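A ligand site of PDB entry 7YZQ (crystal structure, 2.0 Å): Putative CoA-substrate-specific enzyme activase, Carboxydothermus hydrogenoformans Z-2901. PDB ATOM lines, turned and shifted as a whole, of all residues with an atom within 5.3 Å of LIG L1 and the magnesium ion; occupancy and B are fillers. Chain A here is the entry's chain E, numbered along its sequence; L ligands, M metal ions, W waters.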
ATOM      1  N   ASP A   6      16.592  -4.834 -27.070  1.00  0.00           N
ATOM      2  CA  ASP A   6      17.992  -4.666 -26.707  1.00  0.00           C
ATOM      3  C   ASP A   6      18.273  -5.677 -25.615  1.00  0.00           C
ATOM      4  O   ASP A   6      17.865  -5.494 -24.466  1.00  0.00           O
ATOM      5  CB  ASP A   6      18.274  -3.243 -26.257  1.00  0.00           C
ATOM      6  CG  ASP A   6      19.675  -3.083 -25.721  1.00  0.00           C
ATOM      7  OD1 ASP A   6      20.554  -3.990 -25.973  1.00  0.00           O
ATOM      8  OD2 ASP A   6      19.952  -2.058 -25.082  1.00  0.00           O
ATOM      9  N   GLY A   8      20.763  -6.948 -23.548  1.00  0.00           N
ATOM     10  CA  GLY A   8      22.061  -6.677 -22.983  1.00  0.00           C
ATOM     11  C   GLY A   8      22.517  -7.699 -21.968  1.00  0.00           C
ATOM     12  O   GLY A   8      21.769  -8.580 -21.505  1.00  0.00           O
ATOM     13  N   SER A   9      23.794  -7.563 -21.619  1.00  0.00           N
ATOM     14  CA  SER A   9      24.381  -8.470 -20.653  1.00  0.00           C
ATOM     15  C   SER A   9      23.662  -8.431 -19.319  1.00  0.00           C
ATOM     16  O   SER A   9      23.603  -9.454 -18.645  1.00  0.00           O
ATOM     17  CB  SER A   9      25.870  -8.153 -20.455  1.00  0.00           C
ATOM     18  OG  SER A   9      26.078  -7.031 -19.649  1.00  0.00           O
ATOM     19  N   THR A  10      23.128  -7.273 -18.942  1.00  0.00           N
ATOM     20  CA  THR A  10      22.562  -7.017 -17.632  1.00  0.00           C
ATOM     21  C   THR A  10      21.057  -6.835 -17.677  1.00  0.00           C
ATOM     22  O   THR A  10      20.342  -7.404 -16.847  1.00  0.00           O
ATOM     23  CB  THR A  10      23.217  -5.760 -17.031  1.00  0.00           C
ATOM     24  OG1 THR A  10      24.635  -5.966 -16.908  1.00  0.00           O
ATOM     25  CG2 THR A  10      22.670  -5.470 -15.688  1.00  0.00           C
ATOM     26  N   ASN A  11      20.563  -6.043 -18.624  1.00  0.00           N
ATOM     27  CA  ASN A  11      19.147  -5.720 -18.704  1.00  0.00           C
ATOM     28  C   ASN A  11      18.718  -5.879 -20.137  1.00  0.00           C
ATOM     29  O   ASN A  11      19.491  -5.638 -21.056  1.00  0.00           O
ATOM     30  CB  ASN A  11      18.808  -4.285 -18.266  1.00  0.00           C
ATOM     31  CG  ASN A  11      19.064  -4.078 -16.782  1.00  0.00           C
ATOM     32  OD1 ASN A  11      18.507  -4.773 -15.937  1.00  0.00           O
ATOM     33  ND2 ASN A  11      20.009  -3.239 -16.478  1.00  0.00           N
ATOM     34  N   LYS A  13      15.699  -4.683 -22.855  1.00  0.00           N
ATOM     35  CA  LYS A  13      14.805  -3.549 -23.015  1.00  0.00           C
ATOM     36  C   LYS A  13      14.067  -3.673 -24.334  1.00  0.00           C
ATOM     37  O   LYS A  13      14.623  -4.147 -25.330  1.00  0.00           O
ATOM     38  CB  LYS A  13      15.572  -2.185 -22.960  1.00  0.00           C
ATOM     39  CG  LYS A  13      16.635  -2.039 -21.929  1.00  0.00           C
ATOM     40  CD  LYS A  13      17.912  -2.825 -22.322  1.00  0.00           C
ATOM     41  CE  LYS A  13      19.105  -2.282 -21.774  1.00  0.00           C
ATOM     42  NZ  LYS A  13      20.237  -3.181 -21.941  1.00  0.00           N
ATOM     43  N   THR A  30      18.232  -9.255 -17.570  1.00  0.00           N
ATOM     44  CA  THR A  30      18.484 -10.335 -18.513  1.00  0.00           C
ATOM     45  C   THR A  30      18.579 -11.684 -17.792  1.00  0.00           C
ATOM     46  O   THR A  30      18.206 -12.728 -18.349  1.00  0.00           O
ATOM     47  CB  THR A  30      19.758 -10.051 -19.293  1.00  0.00           C
ATOM     48  OG1 THR A  30      19.631  -8.792 -19.940  1.00  0.00           O
ATOM     49  CG2 THR A  30      20.042 -11.174 -20.319  1.00  0.00           C
ATOM     50  N   GLU A  69      24.505  -2.846 -31.022  1.00  0.00           N
ATOM     51  CA  GLU A  69      24.189  -1.797 -30.063  1.00  0.00           C
ATOM     52  C   GLU A  69      24.875  -0.494 -30.401  1.00  0.00           C
ATOM     53  O   GLU A  69      24.417   0.536 -29.923  1.00  0.00           O
ATOM     54  CB  GLU A  69      24.550  -2.256 -28.623  1.00  0.00           C
ATOM     55  CG  GLU A  69      26.033  -2.504 -28.328  1.00  0.00           C
ATOM     56  CD  GLU A  69      26.271  -3.446 -27.161  1.00  0.00           C
ATOM     57  OE1 GLU A  69      26.517  -2.960 -26.021  1.00  0.00           O
ATOM     58  OE2 GLU A  69      26.180  -4.682 -27.346  1.00  0.00           O
ATOM     59  N   ASP A  89      28.025   5.541 -23.743  1.00  0.00           N
ATOM     60  CA  ASP A  89      27.114   4.492 -23.268  1.00  0.00           C
ATOM     61  C   ASP A  89      27.911   3.597 -22.319  1.00  0.00           C
ATOM     62  O   ASP A  89      28.863   2.915 -22.748  1.00  0.00           O
ATOM     63  CB  ASP A  89      26.568   3.723 -24.482  1.00  0.00           C
ATOM     64  CG  ASP A  89      25.898   2.425 -24.140  1.00  0.00           C
ATOM     65  OD1 ASP A  89      25.956   1.969 -22.960  1.00  0.00           O
ATOM     66  OD2 ASP A  89      25.318   1.842 -25.101  1.00  0.00           O
ATOM     67  N   LEU A  90      27.506   3.588 -21.057  1.00  0.00           N
ATOM     68  CA  LEU A  90      28.095   2.718 -20.042  1.00  0.00           C
ATOM     69  C   LEU A  90      27.065   1.661 -19.692  1.00  0.00           C
ATOM     70  O   LEU A  90      26.029   1.968 -19.100  1.00  0.00           O
ATOM     71  CB  LEU A  90      28.513   3.497 -18.791  1.00  0.00           C
ATOM     72  CG  LEU A  90      29.165   2.643 -17.726  1.00  0.00           C
ATOM     73  CD1 LEU A  90      30.346   1.847 -18.286  1.00  0.00           C
ATOM     74  CD2 LEU A  90      29.619   3.416 -16.466  1.00  0.00           C
ATOM     75  N   GLY A  91      27.375   0.415 -20.019  1.00  0.00           N
ATOM     76  CA  GLY A  91      26.549  -0.712 -19.698  1.00  0.00           C
ATOM     77  C   GLY A  91      27.193  -1.547 -18.621  1.00  0.00           C
ATOM     78  O   GLY A  91      28.121  -1.104 -17.941  1.00  0.00           O
ATOM     79  N   GLY A  92      26.684  -2.772 -18.454  1.00  0.00           N
ATOM     80  CA  GLY A  92      27.198  -3.626 -17.401  1.00  0.00           C
ATOM     81  C   GLY A  92      28.546  -4.255 -17.729  1.00  0.00           C
ATOM     82  O   GLY A  92      29.374  -4.491 -16.831  1.00  0.00           O
ATOM     83  N   GLN A  93      28.832  -4.490 -18.998  1.00  0.00           N
ATOM     84  CA  GLN A  93      30.088  -5.107 -19.410  1.00  0.00           C
ATOM     85  C   GLN A  93      30.922  -4.279 -20.373  1.00  0.00           C
ATOM     86  O   GLN A  93      32.142  -4.476 -20.423  1.00  0.00           O
ATOM     87  CB  GLN A  93      29.767  -6.495 -20.009  1.00  0.00           C
ATOM     88  CG  GLN A  93      30.802  -7.077 -20.941  1.00  0.00           C
ATOM     89  CD  GLN A  93      31.959  -7.736 -20.248  1.00  0.00           C
ATOM     90  OE1 GLN A  93      32.010  -7.946 -19.002  1.00  0.00           O
ATOM     91  NE2 GLN A  93      32.947  -8.046 -21.059  1.00  0.00           N
ATOM     92  N   LYS A  96      31.179   2.377 -24.388  1.00  0.00           N
ATOM     93  CA  LYS A  96      31.214   2.765 -25.790  1.00  0.00           C
ATOM     94  C   LYS A  96      31.257   4.284 -25.924  1.00  0.00           C
ATOM     95  O   LYS A  96      30.466   4.998 -25.291  1.00  0.00           O
ATOM     96  CB  LYS A  96      30.004   2.204 -26.545  1.00  0.00           C
ATOM     97  CG  LYS A  96      29.554   0.832 -26.173  1.00  0.00           C
ATOM     98  CD  LYS A  96      28.817   0.780 -24.867  1.00  0.00           C
ATOM     99  CE  LYS A  96      28.226  -0.563 -24.572  1.00  0.00           C
ATOM    100  NZ  LYS A  96      27.332  -0.641 -23.397  1.00  0.00           N
ATOM    101  N   GLY A 120      30.595  -1.449 -15.308  1.00  0.00           N
ATOM    102  CA  GLY A 120      29.266  -1.182 -14.783  1.00  0.00           C
ATOM    103  C   GLY A 120      28.815  -2.231 -13.795  1.00  0.00           C
ATOM    104  O   GLY A 120      28.271  -1.908 -12.736  1.00  0.00           O
ATOM    105  N   ARG A 121      29.082  -3.503 -14.092  1.00  0.00           N
ATOM    106  CA  ARG A 121      28.657  -4.588 -13.219  1.00  0.00           C
ATOM    107  C   ARG A 121      29.421  -4.553 -11.913  1.00  0.00           C
ATOM    108  O   ARG A 121      28.877  -4.874 -10.849  1.00  0.00           O
ATOM    109  CB  ARG A 121      28.857  -5.926 -13.935  1.00  0.00           C
ATOM    110  CG  ARG A 121      28.800  -7.126 -13.063  1.00  0.00           C
ATOM    111  CD  ARG A 121      27.375  -7.606 -12.862  1.00  0.00           C
ATOM    112  NE  ARG A 121      27.342  -8.778 -11.969  1.00  0.00           N
ATOM    113  CZ  ARG A 121      26.397  -9.020 -11.049  1.00  0.00           C
ATOM    114  NH1 ARG A 121      25.365  -8.197 -10.881  1.00  0.00           N
ATOM    115  NH2 ARG A 121      26.503 -10.104 -10.281  1.00  0.00           N
ATOM    116  N   LEU A 123      30.548  -1.723 -10.528  1.00  0.00           N
ATOM    117  CA  LEU A 123      29.907  -0.634  -9.782  1.00  0.00           C
ATOM    118  C   LEU A 123      28.629  -1.130  -9.131  1.00  0.00           C
ATOM    119  O   LEU A 123      28.385  -0.883  -7.943  1.00  0.00           O
ATOM    120  CB  LEU A 123      29.597   0.565 -10.686  1.00  0.00           C
ATOM    121  CG  LEU A 123      30.802   1.377 -11.156  1.00  0.00           C
ATOM    122  CD1 LEU A 123      30.420   2.346 -12.216  1.00  0.00           C
ATOM    123  CD2 LEU A 123      31.459   2.088  -9.978  1.00  0.00           C
ATOM    124  N   GLU A 124      27.795  -1.847  -9.897  1.00  0.00           N
ATOM    125  CA  GLU A 124      26.554  -2.391  -9.341  1.00  0.00           C
ATOM    126  C   GLU A 124      26.839  -3.285  -8.122  1.00  0.00           C
ATOM    127  O   GLU A 124      26.173  -3.185  -7.083  1.00  0.00           O
ATOM    128  CB  GLU A 124      25.811  -3.184 -10.435  1.00  0.00           C
ATOM    129  CG  GLU A 124      24.439  -3.673 -10.050  1.00  0.00           C
ATOM    130  CD  GLU A 124      23.825  -4.637 -11.092  1.00  0.00           C
ATOM    131  OE1 GLU A 124      24.587  -5.226 -11.909  1.00  0.00           O
ATOM    132  OE2 GLU A 124      22.576  -4.805 -11.105  1.00  0.00           O
ATOM    133  N   GLY A 202      22.921   4.766 -21.275  1.00  0.00           N
ATOM    134  CA  GLY A 202      23.033   3.467 -20.672  1.00  0.00           C
ATOM    135  C   GLY A 202      22.781   3.548 -19.187  1.00  0.00           C
ATOM    136  O   GLY A 202      22.661   4.615 -18.605  1.00  0.00           O
ATOM    137  N   GLY A 203      22.637   2.371 -18.552  1.00  0.00           N
ATOM    138  CA  GLY A 203      22.355   2.321 -17.130  1.00  0.00           C
ATOM    139  C   GLY A 203      23.409   2.956 -16.247  1.00  0.00           C
ATOM    140  O   GLY A 203      23.083   3.482 -15.172  1.00  0.00           O
ATOM    141  N   GLY A 204      24.668   2.903 -16.647  1.00  0.00           N
ATOM    142  CA  GLY A 204      25.721   3.562 -15.884  1.00  0.00           C
ATOM    143  C   GLY A 204      25.499   5.052 -15.721  1.00  0.00           C
ATOM    144  O   GLY A 204      25.952   5.652 -14.735  1.00  0.00           O
ATOM    145  N   LYS A 206      22.865   6.368 -14.837  1.00  0.00           N
ATOM    146  CA  LYS A 206      21.835   6.563 -13.817  1.00  0.00           C
ATOM    147  C   LYS A 206      22.454   6.780 -12.441  1.00  0.00           C
ATOM    148  O   LYS A 206      21.720   6.921 -11.465  1.00  0.00           O
ATOM    149  CB  LYS A 206      20.874   5.374 -13.793  1.00  0.00           C
ATOM    150  CG  LYS A 206      20.196   5.083 -15.130  1.00  0.00           C
ATOM    151  CD  LYS A 206      19.112   4.014 -15.038  1.00  0.00           C
ATOM    152  CE  LYS A 206      17.723   4.616 -15.315  1.00  0.00           C
ATOM    153  NZ  LYS A 206      16.680   3.635 -15.644  1.00  0.00           N
ATOM    154  N   TYR A 207      23.771   6.811 -12.333  1.00  0.00           N
ATOM    155  CA  TYR A 207      24.465   7.180 -11.096  1.00  0.00           C
ATOM    156  C   TYR A 207      24.730   8.684 -11.120  1.00  0.00           C
ATOM    157  O   TYR A 207      25.661   9.132 -11.805  1.00  0.00           O
ATOM    158  CB  TYR A 207      25.786   6.430 -10.930  1.00  0.00           C
ATOM    159  CG  TYR A 207      25.681   4.916 -10.772  1.00  0.00           C
ATOM    160  CD1 TYR A 207      24.989   4.344  -9.715  1.00  0.00           C
ATOM    161  CD2 TYR A 207      26.335   4.058 -11.663  1.00  0.00           C
ATOM    162  CE1 TYR A 207      24.905   2.968  -9.568  1.00  0.00           C
ATOM    163  CE2 TYR A 207      26.263   2.700 -11.511  1.00  0.00           C
ATOM    164  CZ  TYR A 207      25.557   2.154 -10.473  1.00  0.00           C
ATOM    165  OH  TYR A 207      25.515   0.788 -10.332  1.00  0.00           O
ATOM    166  N   SER A 229      18.279   3.912 -19.910  1.00  0.00           N
ATOM    167  CA  SER A 229      18.276   2.458 -20.119  1.00  0.00           C
ATOM    168  C   SER A 229      17.808   2.084 -21.518  1.00  0.00           C
ATOM    169  O   SER A 229      18.290   1.097 -22.084  1.00  0.00           O
ATOM    170  CB  SER A 229      17.400   1.757 -19.077  1.00  0.00           C
ATOM    171  OG  SER A 229      17.940   1.909 -17.782  1.00  0.00           O
HETATM  172  P1  LIG L   1      23.531  -3.496 -20.580  1.00  0.00           P
HETATM  173  O1  LIG L   1      22.909  -2.786 -21.761  1.00  0.00           O
HETATM  174  O2  LIG L   1      22.721  -4.758 -20.209  1.00  0.00           O
HETATM  175  O3  LIG L   1      25.009  -3.705 -20.716  1.00  0.00           O
HETATM  176  P2  LIG L   1      22.532  -1.273 -18.942  1.00  0.00           P
HETATM  177  O4  LIG L   1      22.752  -0.204 -20.004  1.00  0.00           O
HETATM  178  O5  LIG L   1      21.191  -1.913 -18.737  1.00  0.00           O
HETATM  179  O6  LIG L   1      23.538  -2.526 -19.264  1.00  0.00           O
HETATM  180  O7  LIG L   1      23.170  -0.788 -17.575  1.00  0.00           O
HETATM  181  C1  LIG L   1      23.429  -1.701 -16.548  1.00  0.00           C
HETATM  182  C2  LIG L   1      24.188  -0.919 -15.502  1.00  0.00           C
HETATM  183  O8  LIG L   1      23.389   0.190 -14.977  1.00  0.00           O
HETATM  184  C3  LIG L   1      24.685  -1.684 -14.257  1.00  0.00           C
HETATM  185  O9  LIG L   1      25.906  -2.398 -14.507  1.00  0.00           O
HETATM  186  C4  LIG L   1      24.861  -0.520 -13.250  1.00  0.00           C
HETATM  187  O10 LIG L   1      26.250  -0.169 -13.317  1.00  0.00           O
HETATM  188  C5  LIG L   1      24.018   0.651 -13.744  1.00  0.00           C
HETATM  189  N1  LIG L   1      23.013   1.079 -12.723  1.00  0.00           N
HETATM  190  C6  LIG L   1      22.781   2.383 -12.378  1.00  0.00           C
HETATM  191  N2  LIG L   1      21.852   2.466 -11.397  1.00  0.00           N
HETATM  192  C7  LIG L   1      21.446   1.215 -11.128  1.00  0.00           C
HETATM  193  C8  LIG L   1      20.513   0.574 -10.188  1.00  0.00           C
HETATM  194  N3  LIG L   1      19.761   1.326  -9.357  1.00  0.00           N
HETATM  195  N4  LIG L   1      20.427  -0.773 -10.182  1.00  0.00           N
HETATM  196  C9  LIG L   1      21.168  -1.557 -10.984  1.00  0.00           C
HETATM  197  N5  LIG L   1      22.064  -1.043 -11.866  1.00  0.00           N
HETATM  198  C10 LIG L   1      22.231   0.296 -11.988  1.00  0.00           C
HETATM  199 AL1  LG2 L   2      26.180  -4.129 -22.177  1.00  0.00          AL
HETATM  200  F1  LG2 L   2      27.375  -2.913 -21.648  1.00  0.00           F
HETATM  201  F2  LG2 L   2      25.025  -5.312 -22.917  1.00  0.00           F
HETATM  202  F3  LG2 L   2      25.391  -2.852 -23.088  1.00  0.00           F
HETATM  203  F4  LG2 L   2      27.052  -5.414 -21.339  1.00  0.00           F
HETATM  204 MG    MG M   1      23.763  -1.822 -23.496  1.00  0.00          MG
HETATM  205  O   HOH W   1      21.890  -0.915 -23.853  1.00  0.00           O
HETATM  206  O   HOH W   2      21.185  -3.330 -13.427  1.00  0.00           O
HETATM  207  O   HOH W   3      23.024  -3.313 -24.807  1.00  0.00           O
HETATM  208  O   HOH W   4      20.574   0.221 -14.765  1.00  0.00           O
HETATM  209  O   HOH W   5      20.913   0.645 -21.883  1.00  0.00           O
HETATM  210  O   HOH W   6      20.841   4.581  -9.551  1.00  0.00           O
HETATM  211  O   HOH W   7      23.592   0.201  -8.696  1.00  0.00           O
HETATM  212  O   HOH W   8      19.820  -0.064 -17.255  1.00  0.00           O
HETATM  213  O   HOH W   9      22.079   1.395  -6.875  1.00  0.00           O
HETATM  214  O   HOH W  10      25.575  -5.186 -14.309  1.00  0.00           O
HETATM  215  O   HOH W  11      24.850  -0.812 -25.056  1.00  0.00           O
HETATM  216  O   HOH W  12      24.304  -0.207 -22.089  1.00  0.00           O
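The side-chain amino group of Lys 13 lies within salt-bridge range of an oxygen (O2) of LIG L1. The backbone carbonyl oxygen (O) of Gly 120 lies within hydrogen-bond range of an oxygen (O10) of LIG L1, 2.7 Å away. An oxygen (O2) of LIG L1 sits at hydrogen-bond distance from the backbone NH of Thr 10 (2.8 Å). N of Asn 11 is in hydrogen-bond range of O2 of LIG L1, 3.0 Å away. ND2 of Asn 11 is in hydrogen-bond range of O5 of LIG L1, 2.9 Å away. The backbone NH (N) of Gly 203 is in hydrogen-bond range of an oxygen (O4) of LIG L1. O6 of LIG L1 lies within hydrogen-bond range of N of Gly 92 (3.3 Å). The side-chain hydroxyl (OH) of Tyr 207 sits at hydrogen-bond distance from an oxygen (O10) of LIG L1 (3.2 Å). The backbone NH (N) of Ser 9 is in hydrogen-bond range of an oxygen (O2) of LIG L1. The backbone NH of Arg 121 lies within hydrogen-bond range of an oxygen (O9) of LIG L1 (3.4 Å). The backbone NH (N) of Gly 204 is in hydrogen-bond range of an oxygen (O8) of LIG L1, at 3.4 Å. The backbone NH (N) of Gly 92 sits at hydrogen-bond distance from a fluorine (F1) of LG2 L2 (3.3 Å). F2 of LG2 L2 is in hydrogen-bond range of N of Ser 9. F4 of LG2 L2 lies within hydrogen-bond range of OG of Ser 9, at 2.5 Å. The side-chain amino group (NZ) of Lys 96 lies within hydrogen-bond range of a fluorine (F1) of LG2 L2, 2.9 Å away. N of Gln 93 sits at hydrogen-bond distance from F4 of LG2 L2 (3.1 Å).
An aluminium atom (AL1) of LG2 L2 is bound by an oxygen (O3) of LIG L1 (1.9 Å).
NZ of Lys 13 is in hydrogen-bond range of O of Asn 11, at 2.7 Å. OG of Ser 9 is in hydrogen-bond range of OG1 of Thr 10 (3.3 Å). The backbone carbonyl oxygen (O) of Thr 10 sits at hydrogen-bond distance from the backbone NH (N) of Thr 30 (2.9 Å). The side-chain hydroxyl (OG1) of Thr 30 sits close to the backbone NH (N) of Asn 11. N of Gly 203 lies within hydrogen-bond range of O of Leu 90 (3.5 Å). The backbone carbonyl oxygen of Gly 92 sits at hydrogen-bond distance from the backbone NH of Arg 121 (2.9 Å). OE1 of Glu 124 is in salt-bridge range of NH1 of Arg 121, 3.2 Å away. The backbone carbonyl oxygen (O) of Leu 90 lies within hydrogen-bond range of the backbone NH (N) of Gly 204, at 3.0 Å.
Merely in contact with LIG L1: Gly 8, Gly 91, Glu 124, Gly 202 and Lys 206.
OE1 of Glu 69 touches the magnesium ion, 3.9 Å away. Lys 96 touches the magnesium ion. Of the 24 residues printed, 2 come within 4 Å of the magnesium ion.
The magnesium ion is bound by F3 of LG2 L2 (2.0 Å), water W1 (2.1 Å), water W3 (2.1 Å), water W11 (2.2 Å), O1 of LIG L1 (2.2 Å) and water W12 (2.2 Å). The magnesium ion has six donor atoms within binding distance.
Water W1 bridges OD2 of Asp 6 (2.6 Å) and NZ of Lys 13 (3.4 Å). Water W11 lies within hydrogen-bond range of the side-chain carboxylate of Asp 89, the side-chain carboxylate of Glu 69 and the side-chain amino group of Lys 96. Water W5 lies within hydrogen-bond range of O of Ser 229 (2.7 Å) and O4 of LIG L1 (2.8 Å). Water W10 lies within hydrogen-bond range of OE1 of Glu 124 (2.6 Å), O9 of LIG L1 (2.8 Å) and OG1 of Thr 10 (2.9 Å). Water W2 lies within hydrogen-bond range of a nitrogen (N5) of LIG L1 (2.9 Å), the side-chain carboxylate (OE2) of Glu 124 (3.1 Å) and the side-chain amide nitrogen (ND2) of Asn 11 (3.3 Å). Water W6 lies within hydrogen-bond range of a nitrogen (N2) of LIG L1 (3.0 Å) and the backbone carbonyl oxygen (O) of Lys 206 (3.1 Å).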
